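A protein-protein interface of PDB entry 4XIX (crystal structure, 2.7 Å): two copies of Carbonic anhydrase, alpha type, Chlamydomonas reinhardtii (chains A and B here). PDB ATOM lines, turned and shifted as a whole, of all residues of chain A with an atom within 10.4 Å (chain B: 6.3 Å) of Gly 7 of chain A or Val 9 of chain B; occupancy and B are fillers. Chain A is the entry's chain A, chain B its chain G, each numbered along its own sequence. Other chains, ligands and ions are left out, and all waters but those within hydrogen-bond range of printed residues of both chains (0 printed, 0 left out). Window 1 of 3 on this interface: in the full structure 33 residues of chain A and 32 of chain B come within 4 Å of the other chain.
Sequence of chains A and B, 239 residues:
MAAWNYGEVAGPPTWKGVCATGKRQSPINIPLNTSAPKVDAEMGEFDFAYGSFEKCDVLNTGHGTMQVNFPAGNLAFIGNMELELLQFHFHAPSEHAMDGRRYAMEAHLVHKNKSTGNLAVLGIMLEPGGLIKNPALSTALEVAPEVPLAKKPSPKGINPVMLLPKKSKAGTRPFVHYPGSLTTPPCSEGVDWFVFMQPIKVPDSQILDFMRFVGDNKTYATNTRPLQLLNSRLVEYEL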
ATOM      1  N   ALA A   3     -20.413  23.495  27.972  1.00  0.00           N
ATOM      2  CA  ALA A   3     -20.747  22.082  27.806  1.00  0.00           C
ATOM      3  C   ALA A   3     -19.843  21.429  26.749  1.00  0.00           C
ATOM      4  O   ALA A   3     -20.324  20.698  25.887  1.00  0.00           O
ATOM      5  CB  ALA A   3     -22.238  21.916  27.445  1.00  0.00           C
ATOM      6  N   TRP A   4     -18.534  21.693  26.823  1.00  0.00           N
ATOM      7  CA  TRP A   4     -17.562  21.026  25.961  1.00  0.00           C
ATOM      8  C   TRP A   4     -16.628  20.156  26.787  1.00  0.00           C
ATOM      9  O   TRP A   4     -16.283  20.497  27.920  1.00  0.00           O
ATOM     10  CB  TRP A   4     -16.755  22.038  25.137  1.00  0.00           C
ATOM     11  CG  TRP A   4     -15.725  22.801  25.898  1.00  0.00           C
ATOM     12  CD1 TRP A   4     -15.870  24.021  26.447  1.00  0.00           C
ATOM     13  CD2 TRP A   4     -14.386  22.393  26.180  1.00  0.00           C
ATOM     14  NE1 TRP A   4     -14.708  24.423  27.064  1.00  0.00           N
ATOM     15  CE2 TRP A   4     -13.777  23.436  26.915  1.00  0.00           C
ATOM     16  CE3 TRP A   4     -13.638  21.247  25.883  1.00  0.00           C
ATOM     17  CZ2 TRP A   4     -12.455  23.368  27.364  1.00  0.00           C
ATOM     18  CZ3 TRP A   4     -12.320  21.181  26.323  1.00  0.00           C
ATOM     19  CH2 TRP A   4     -11.744  22.237  27.057  1.00  0.00           C
ATOM     20  N   ASN A   5     -16.232  19.023  26.214  1.00  0.00           N
ATOM     21  CA  ASN A   5     -15.251  18.158  26.857  1.00  0.00           C
ATOM     22  C   ASN A   5     -14.324  17.483  25.875  1.00  0.00           C
ATOM     23  O   ASN A   5     -14.498  17.536  24.671  1.00  0.00           O
ATOM     24  CB  ASN A   5     -15.905  17.089  27.761  1.00  0.00           C
ATOM     25  CG  ASN A   5     -16.774  16.077  27.000  1.00  0.00           C
ATOM     26  OD1 ASN A   5     -16.717  15.928  25.776  1.00  0.00           O
ATOM     27  ND2 ASN A   5     -17.582  15.362  27.753  1.00  0.00           N
ATOM     28  N   TYR A   6     -13.304  16.849  26.406  1.00  0.00           N
ATOM     29  CA  TYR A   6     -12.614  15.889  25.607  1.00  0.00           C
ATOM     30  C   TYR A   6     -13.472  14.600  25.562  1.00  0.00           C
ATOM     31  O   TYR A   6     -13.954  14.210  24.507  1.00  0.00           O
ATOM     32  CB  TYR A   6     -11.234  15.687  26.179  1.00  0.00           C
ATOM     33  CG  TYR A   6     -10.405  16.913  26.086  1.00  0.00           C
ATOM     34  CD1 TYR A   6      -9.770  17.251  24.896  1.00  0.00           C
ATOM     35  CD2 TYR A   6     -10.251  17.755  27.187  1.00  0.00           C
ATOM     36  CE1 TYR A   6      -8.994  18.409  24.806  1.00  0.00           C
ATOM     37  CE2 TYR A   6      -9.484  18.902  27.104  1.00  0.00           C
ATOM     38  CZ  TYR A   6      -8.861  19.223  25.910  1.00  0.00           C
ATOM     39  OH  TYR A   6      -8.097  20.357  25.819  1.00  0.00           O
ATOM     40  N   GLY A   7     -13.710  13.980  26.712  1.00  0.00           N
ATOM     41  CA  GLY A   7     -14.592  12.831  26.787  1.00  0.00           C
ATOM     42  C   GLY A   7     -13.796  11.560  26.605  1.00  0.00           C
ATOM     43  O   GLY A   7     -12.569  11.619  26.538  1.00  0.00           O
ATOM     44  N   GLU A   8     -14.482  10.421  26.524  1.00  0.00           N
ATOM     45  CA  GLU A   8     -13.801   9.130  26.401  1.00  0.00           C
ATOM     46  C   GLU A   8     -13.578   8.812  24.957  1.00  0.00           C
ATOM     47  O   GLU A   8     -14.223   9.393  24.093  1.00  0.00           O
ATOM     48  CB  GLU A   8     -14.598   7.986  27.043  1.00  0.00           C
ATOM     49  CG  GLU A   8     -14.849   8.163  28.511  1.00  0.00           C
ATOM     50  CD  GLU A   8     -13.621   8.671  29.261  1.00  0.00           C
ATOM     51  OE1 GLU A   8     -12.481   8.174  29.011  1.00  0.00           O
ATOM     52  OE2 GLU A   8     -13.801   9.593  30.094  1.00  0.00           O
ATOM     53  N   VAL A   9     -12.659   7.888  24.704  1.00  0.00           N
ATOM     54  CA  VAL A   9     -12.413   7.428  23.353  1.00  0.00           C
ATOM     55  C   VAL A   9     -13.761   7.095  22.654  1.00  0.00           C
ATOM     56  O   VAL A   9     -14.682   6.570  23.272  1.00  0.00           O
ATOM     57  CB  VAL A   9     -11.406   6.243  23.345  1.00  0.00           C
ATOM     58  CG1 VAL A   9     -10.054   6.714  23.799  1.00  0.00           C
ATOM     59  CG2 VAL A   9     -11.868   5.120  24.238  1.00  0.00           C
ATOM     60  N   ALA A  10     -13.897   7.469  21.387  1.00  0.00           N
ATOM     61  CA  ALA A  10     -15.155   7.266  20.672  1.00  0.00           C
ATOM     62  C   ALA A  10     -15.412   5.788  20.327  1.00  0.00           C
ATOM     63  O   ALA A  10     -16.521   5.431  19.950  1.00  0.00           O
ATOM     64  CB  ALA A  10     -15.180   8.119  19.404  1.00  0.00           C
ATOM     65  N   GLY A  11     -14.393   4.939  20.452  1.00  0.00           N
ATOM     66  CA  GLY A  11     -14.487   3.575  19.965  1.00  0.00           C
ATOM     67  C   GLY A  11     -15.556   2.717  20.637  1.00  0.00           C
ATOM     68  O   GLY A  11     -16.604   2.425  20.052  1.00  0.00           O
ATOM     69  N   PRO A  12     -15.294   2.297  21.881  1.00  0.00           N
ATOM     70  CA  PRO A  12     -16.119   1.298  22.557  1.00  0.00           C
ATOM     71  C   PRO A  12     -17.617   1.521  22.483  1.00  0.00           C
ATOM     72  O   PRO A  12     -18.358   0.577  22.231  1.00  0.00           O
ATOM     73  CB  PRO A  12     -15.609   1.355  23.999  1.00  0.00           C
ATOM     74  CG  PRO A  12     -14.162   1.647  23.839  1.00  0.00           C
ATOM     75  CD  PRO A  12     -14.104   2.640  22.679  1.00  0.00           C
ATOM     76  N   PRO A  13     -18.070   2.749  22.675  1.00  0.00           N
ATOM     77  CA  PRO A  13     -19.533   2.863  22.653  1.00  0.00           C
ATOM     78  C   PRO A  13     -20.183   2.586  21.282  1.00  0.00           C
ATOM     79  O   PRO A  13     -21.400   2.437  21.227  1.00  0.00           O
ATOM     80  CB  PRO A  13     -19.785   4.296  23.126  1.00  0.00           C
ATOM     81  CG  PRO A  13     -18.455   5.012  22.990  1.00  0.00           C
ATOM     82  CD  PRO A  13     -17.392   3.994  23.085  1.00  0.00           C
ATOM     83  N   THR A  14     -19.401   2.476  20.212  1.00  0.00           N
ATOM     84  CA  THR A  14     -19.948   2.097  18.902  1.00  0.00           C
ATOM     85  C   THR A  14     -19.841   0.593  18.601  1.00  0.00           C
ATOM     86  O   THR A  14     -20.326   0.129  17.564  1.00  0.00           O
ATOM     87  CB  THR A  14     -19.197   2.768  17.770  1.00  0.00           C
ATOM     88  OG1 THR A  14     -18.041   1.977  17.439  1.00  0.00           O
ATOM     89  CG2 THR A  14     -18.780   4.186  18.154  1.00  0.00           C
ATOM     90  N   ARG A 102      -9.000   3.588  38.727  1.00  0.00           N
ATOM     91  CA  ARG A 102      -8.218   2.743  37.827  1.00  0.00           C
ATOM     92  C   ARG A 102      -6.728   2.908  38.054  1.00  0.00           C
ATOM     93  O   ARG A 102      -6.284   3.941  38.505  1.00  0.00           O
ATOM     94  CB  ARG A 102      -8.553   3.044  36.377  1.00  0.00           C
ATOM     95  CG  ARG A 102      -9.886   2.553  35.986  1.00  0.00           C
ATOM     96  CD  ARG A 102     -10.143   2.820  34.550  1.00  0.00           C
ATOM     97  NE  ARG A 102     -11.088   1.854  34.013  1.00  0.00           N
ATOM     98  CZ  ARG A 102     -11.743   1.997  32.864  1.00  0.00           C
ATOM     99  NH1 ARG A 102     -11.565   3.075  32.122  1.00  0.00           N
ATOM    100  NH2 ARG A 102     -12.583   1.052  32.456  1.00  0.00           N
ATOM    101  N   TYR A 220       0.913   9.130  22.843  1.00  0.00           N
ATOM    102  CA  TYR A 220       0.612   8.325  24.013  1.00  0.00           C
ATOM    103  C   TYR A 220      -0.882   8.093  23.966  1.00  0.00           C
ATOM    104  O   TYR A 220      -1.639   9.034  23.774  1.00  0.00           O
ATOM    105  CB  TYR A 220       1.064   9.031  25.294  1.00  0.00           C
ATOM    106  CG  TYR A 220       2.571   9.136  25.413  1.00  0.00           C
ATOM    107  CD1 TYR A 220       3.279  10.167  24.773  1.00  0.00           C
ATOM    108  CD2 TYR A 220       3.303   8.210  26.150  1.00  0.00           C
ATOM    109  CE1 TYR A 220       4.698  10.272  24.865  1.00  0.00           C
ATOM    110  CE2 TYR A 220       4.721   8.301  26.253  1.00  0.00           C
ATOM    111  CZ  TYR A 220       5.409   9.342  25.612  1.00  0.00           C
ATOM    112  OH  TYR A 220       6.793   9.448  25.708  1.00  0.00           O
ATOM    113  N   ALA A 221      -1.308   6.837  24.074  1.00  0.00           N
ATOM    114  CA  ALA A 221      -2.705   6.486  23.852  1.00  0.00           C
ATOM    115  C   ALA A 221      -3.133   5.541  24.918  1.00  0.00           C
ATOM    116  O   ALA A 221      -2.300   5.020  25.657  1.00  0.00           O
ATOM    117  CB  ALA A 221      -2.871   5.818  22.540  1.00  0.00           C
ATOM    118  N   THR A 222      -4.435   5.284  24.951  1.00  0.00           N
ATOM    119  CA  THR A 222      -5.003   4.272  25.836  1.00  0.00           C
ATOM    120  C   THR A 222      -5.709   3.142  25.068  1.00  0.00           C
ATOM    121  O   THR A 222      -5.970   3.268  23.860  1.00  0.00           O
ATOM    122  CB  THR A 222      -5.972   4.923  26.822  1.00  0.00           C
ATOM    123  OG1 THR A 222      -7.122   5.411  26.116  1.00  0.00           O
ATOM    124  CG2 THR A 222      -5.256   6.074  27.561  1.00  0.00           C
ATOM    125  N   THR A 224      -8.404   0.880  26.776  1.00  0.00           N
ATOM    126  CA  THR A 224      -9.271   0.382  27.806  1.00  0.00           C
ATOM    127  C   THR A 224     -10.706   0.680  27.459  1.00  0.00           C
ATOM    128  O   THR A 224     -11.020   1.723  26.900  1.00  0.00           O
ATOM    129  CB  THR A 224      -8.917   1.028  29.148  1.00  0.00           C
ATOM    130  OG1 THR A 224      -7.907   0.239  29.794  1.00  0.00           O
ATOM    131  CG2 THR A 224     -10.122   1.109  30.092  1.00  0.00           C
ATOM    132  N   PRO A 226     -14.732   1.236  28.685  1.00  0.00           N
ATOM    133  CA  PRO A 226     -15.333   1.825  29.885  1.00  0.00           C
ATOM    134  C   PRO A 226     -15.908   0.767  30.835  1.00  0.00           C
ATOM    135  O   PRO A 226     -16.257  -0.322  30.393  1.00  0.00           O
ATOM    136  CB  PRO A 226     -16.451   2.683  29.317  1.00  0.00           C
ATOM    137  CG  PRO A 226     -16.060   2.961  27.946  1.00  0.00           C
ATOM    138  CD  PRO A 226     -15.312   1.773  27.449  1.00  0.00           C
ATOM    139  N   TYR B   6     -10.351   1.587  19.497  1.00  0.00           N
ATOM    140  CA  TYR B   6     -10.651   2.461  20.600  1.00  0.00           C
ATOM    141  C   TYR B   6     -10.899   3.917  20.194  1.00  0.00           C
ATOM    142  O   TYR B   6     -11.785   4.596  20.676  1.00  0.00           O
ATOM    143  CB  TYR B   6      -9.518   2.395  21.575  1.00  0.00           C
ATOM    144  CG  TYR B   6      -9.404   1.068  22.219  1.00  0.00           C
ATOM    145  CD1 TYR B   6     -10.174   0.756  23.272  1.00  0.00           C
ATOM    146  CD2 TYR B   6      -8.556   0.145  21.748  1.00  0.00           C
ATOM    147  CE1 TYR B   6     -10.114  -0.447  23.832  1.00  0.00           C
ATOM    148  CE2 TYR B   6      -8.490  -1.076  22.300  1.00  0.00           C
ATOM    149  CZ  TYR B   6      -9.251  -1.367  23.360  1.00  0.00           C
ATOM    150  OH  TYR B   6      -9.127  -2.564  23.933  1.00  0.00           O
ATOM    151  N   GLY B   7     -10.094   4.378  19.283  1.00  0.00           N
ATOM    152  CA  GLY B   7     -10.232   5.713  18.768  1.00  0.00           C
ATOM    153  C   GLY B   7      -9.602   6.768  19.608  1.00  0.00           C
ATOM    154  O   GLY B   7      -8.745   6.521  20.417  1.00  0.00           O
ATOM    155  N   GLU B   8     -10.059   7.975  19.398  1.00  0.00           N
ATOM    156  CA  GLU B   8      -9.534   9.086  20.111  1.00  0.00           C
ATOM    157  C   GLU B   8     -10.703   9.553  20.829  1.00  0.00           C
ATOM    158  O   GLU B   8     -11.720   8.970  20.681  1.00  0.00           O
ATOM    159  CB  GLU B   8      -8.967  10.102  19.164  1.00  0.00           C
ATOM    160  CG  GLU B   8      -7.742   9.614  18.434  1.00  0.00           C
ATOM    161  CD  GLU B   8      -7.235  10.630  17.435  1.00  0.00           C
ATOM    162  OE1 GLU B   8      -7.943  11.599  17.200  1.00  0.00           O
ATOM    163  OE2 GLU B   8      -6.141  10.496  16.874  1.00  0.00           O
ATOM    164  N   VAL B   9     -10.540  10.542  21.663  1.00  0.00           N
ATOM    165  CA  VAL B   9     -11.643  11.062  22.388  1.00  0.00           C
ATOM    166  C   VAL B   9     -12.706  11.565  21.477  1.00  0.00           C
ATOM    167  O   VAL B   9     -12.468  11.954  20.371  1.00  0.00           O
ATOM    168  CB  VAL B   9     -11.217  12.124  23.375  1.00  0.00           C
ATOM    169  CG1 VAL B   9     -10.541  11.486  24.543  1.00  0.00           C
ATOM    170  CG2 VAL B   9     -10.285  13.105  22.733  1.00  0.00           C
ATOM    171  N   ALA B  10     -13.913  11.516  21.964  1.00  0.00           N
ATOM    172  CA  ALA B  10     -15.067  11.774  21.160  1.00  0.00           C
ATOM    173  C   ALA B  10     -15.543  13.214  21.132  1.00  0.00           C
ATOM    174  O   ALA B  10     -16.420  13.535  20.381  1.00  0.00           O
ATOM    175  CB  ALA B  10     -16.188  10.890  21.633  1.00  0.00           C
ATOM    176  N   GLY B  11     -14.993  14.055  21.978  1.00  0.00           N
ATOM    177  CA  GLY B  11     -15.512  15.405  22.110  1.00  0.00           C
ATOM    178  C   GLY B  11     -15.075  16.363  21.011  1.00  0.00           C
ATOM    179  O   GLY B  11     -15.906  16.929  20.331  1.00  0.00           O
ATOM    180  N   PRO B  12     -13.761  16.539  20.833  1.00  0.00           N
ATOM    181  CA  PRO B  12     -13.239  17.472  19.833  1.00  0.00           C
ATOM    182  C   PRO B  12     -13.922  17.453  18.449  1.00  0.00           C
ATOM    183  O   PRO B  12     -14.306  18.524  17.972  1.00  0.00           O
ATOM    184  CB  PRO B  12     -11.761  17.090  19.752  1.00  0.00           C
ATOM    185  CG  PRO B  12     -11.451  16.560  21.116  1.00  0.00           C
ATOM    186  CD  PRO B  12     -12.676  15.837  21.550  1.00  0.00           C
ATOM    187  N   PRO B  13     -14.089  16.288  17.808  1.00  0.00           N
ATOM    188  CA  PRO B  13     -14.678  16.340  16.455  1.00  0.00           C
ATOM    189  C   PRO B  13     -16.096  16.912  16.401  1.00  0.00           C
ATOM    190  O   PRO B  13     -16.624  17.116  15.311  1.00  0.00           O
ATOM    191  CB  PRO B  13     -14.704  14.870  16.025  1.00  0.00           C
ATOM    192  CG  PRO B  13     -14.565  14.117  17.262  1.00  0.00           C
ATOM    193  CD  PRO B  13     -13.741  14.918  18.193  1.00  0.00           C
ATOM    194  N   THR B 222      -6.078  11.878  28.713  1.00  0.00           N
ATOM    195  CA  THR B 222      -5.435  12.806  27.810  1.00  0.00           C
ATOM    196  C   THR B 222      -6.332  14.037  27.686  1.00  0.00           C
ATOM    197  O   THR B 222      -7.472  13.999  28.141  1.00  0.00           O
ATOM    198  CB  THR B 222      -5.146  12.130  26.442  1.00  0.00           C
ATOM    199  OG1 THR B 222      -6.346  11.557  25.878  1.00  0.00           O
ATOM    200  CG2 THR B 222      -4.080  11.020  26.618  1.00  0.00           C
ATOM    201  N   THR B 224      -6.133  16.470  24.610  1.00  0.00           N
ATOM    202  CA  THR B 224      -5.524  17.018  23.408  1.00  0.00           C
ATOM    203  C   THR B 224      -6.485  16.977  22.237  1.00  0.00           C
ATOM    204  O   THR B 224      -7.224  16.034  22.034  1.00  0.00           O
ATOM    205  CB  THR B 224      -4.234  16.228  23.060  1.00  0.00           C
ATOM    206  OG1 THR B 224      -3.194  16.645  23.938  1.00  0.00           O
ATOM    207  CG2 THR B 224      -3.728  16.510  21.702  1.00  0.00           C
ATOM    208  N   PRO B 226      -7.104  16.787  18.159  1.00  0.00           N
ATOM    209  CA  PRO B 226      -6.399  16.322  16.959  1.00  0.00           C
ATOM    210  C   PRO B 226      -5.700  17.445  16.171  1.00  0.00           C
ATOM    211  O   PRO B 226      -6.016  18.625  16.344  1.00  0.00           O
ATOM    212  CB  PRO B 226      -7.520  15.760  16.101  1.00  0.00           C
ATOM    213  CG  PRO B 226      -8.690  15.665  16.971  1.00  0.00           C
ATOM    214  CD  PRO B 226      -8.555  16.629  18.052  1.00  0.00           C
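The backbone carbonyl oxygen (O) of Gly 11 of chain A lies within hydrogen-bond range of the side-chain hydroxyl (OG1) of Thr 14 of chain A (3.0 Å).
The backbone carbonyl oxygen of Tyr 6 of chain A sits at hydrogen-bond distance from the backbone NH of Gly 11 of chain B, 2.7 Å away. The backbone carbonyl oxygen of Glu 8 of chain A lies within hydrogen-bond range of the backbone NH of Ala 10 of chain B, at 3.0 Å. The backbone carbonyl oxygen (O) of Glu 8 of chain B lies within hydrogen-bond range of the backbone NH (N) of Ala 10 of chain A, at 2.7 Å. O of Tyr 6 of chain B lies within hydrogen-bond range of N of Gly 11 of chain A, 2.6 Å away.
Printed residues of chain B within 4 Å of Tyr 6 of chain A: Val 9, Ala 10, Gly 11, Pro 12 and Thr 224. Printed residues of chain B within 4 Å of Val 9 of chain A: Tyr 6 (3.2 Å), Gly 7 (3.6 Å), Glu 8 (3.2 Å) and Val 9 (3.8 Å). Of the printed residues of chain B, Gly 11 of chain A touches Tyr 6. Printed residues of chain A within 4 Å of Tyr 6 of chain B: Val 9, Ala 10, Gly 11, Pro 12 and Thr 224. Of the printed residues of chain A, Ala 10 of chain B touches Tyr 6 (3.7 Å), Glu 8 (3.0 Å) and Ala 10 (3.7 Å). The nearest printed residue of chain A that does not touch Gly 7 of chain B is Gly 11 of chain A (4.5 Å).
Printed residues of chain A that touch a printed residue of chain B: Asn 5, Tyr 6, Gly 7, Glu 8, Val 9, Ala 10, Gly 11, Pro 12 and Thr 224. Hydrophobic or aromatic side chains of chain A within 4 Å of the printed part of chain B: Tyr 6, Val 9, Ala 10 and Pro 12. Printed residues of chain B that touch a printed residue of chain A: Tyr 6, Gly 7, Glu 8, Val 9, Ala 10, Gly 11, Pro 12 and Thr 224. Hydrophobic or aromatic side chains of chain B within 4 Å of the printed part of chain A: Tyr 6, Val 9, Ala 10 and Pro 12. Among the printed residues, no Asp or Glu carboxylate lies within 4 Å of a Lys or Arg side-chain nitrogen of the other chain.
Among the printed residues, pairs that only touch across the chains: Asn 5 of chain A with Gly 11 of chain B (3.5 Å), Asn 5 of chain A with Pro 12 of chain B (3.99 Å), Tyr 6 of chain A with Val 9 of chain B (3.6 Å), Tyr 6 of chain A with Ala 10 of chain B (3.7 Å), Tyr 6 of chain A with Pro 12 of chain B (3.6 Å), Tyr 6 of chain A with Thr 224 of chain B (3.5 Å), Gly 7 of chain A with Val 9 of chain B (2.8 Å), Glu 8 of chain A with Val 9 of chain B (3.5 Å), Val 9 of chain A with Tyr 6 of chain B (3.2 Å), Val 9 of chain A with Gly 7 of chain B (3.6 Å), Val 9 of chain A with Glu 8 of chain B (3.2 Å), Val 9 of chain A with Val 9 of chain B (3.8 Å), Ala 10 of chain A with Tyr 6 of chain B (3.6 Å), Ala 10 of chain A with Ala 10 of chain B (3.7 Å), Pro 12 of chain A with Tyr 6 of chain B (3.6 Å) and Thr 224 of chain A with Tyr 6 of chain B (3.7 Å).
Tyr 6 of chain A touches Val 9 of chain B, and with the chains exchanged Val 9 of chain A touches Tyr 6 of chain B. Tyr 6 of chain A touches Gly 11 of chain B, and with the chains exchanged Gly 11 of chain A touches Tyr 6 of chain B. Glu 8 of chain A touches Val 9 of chain B, and with the chains exchanged Val 9 of chain A touches Glu 8 of chain B. Val 9 of chain A touches its own counterpart, Val 9 of chain B. Positions printed for both chains: 6, 7, 8, 9, 10, 11, 12, 13, 222, 224 and 226.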
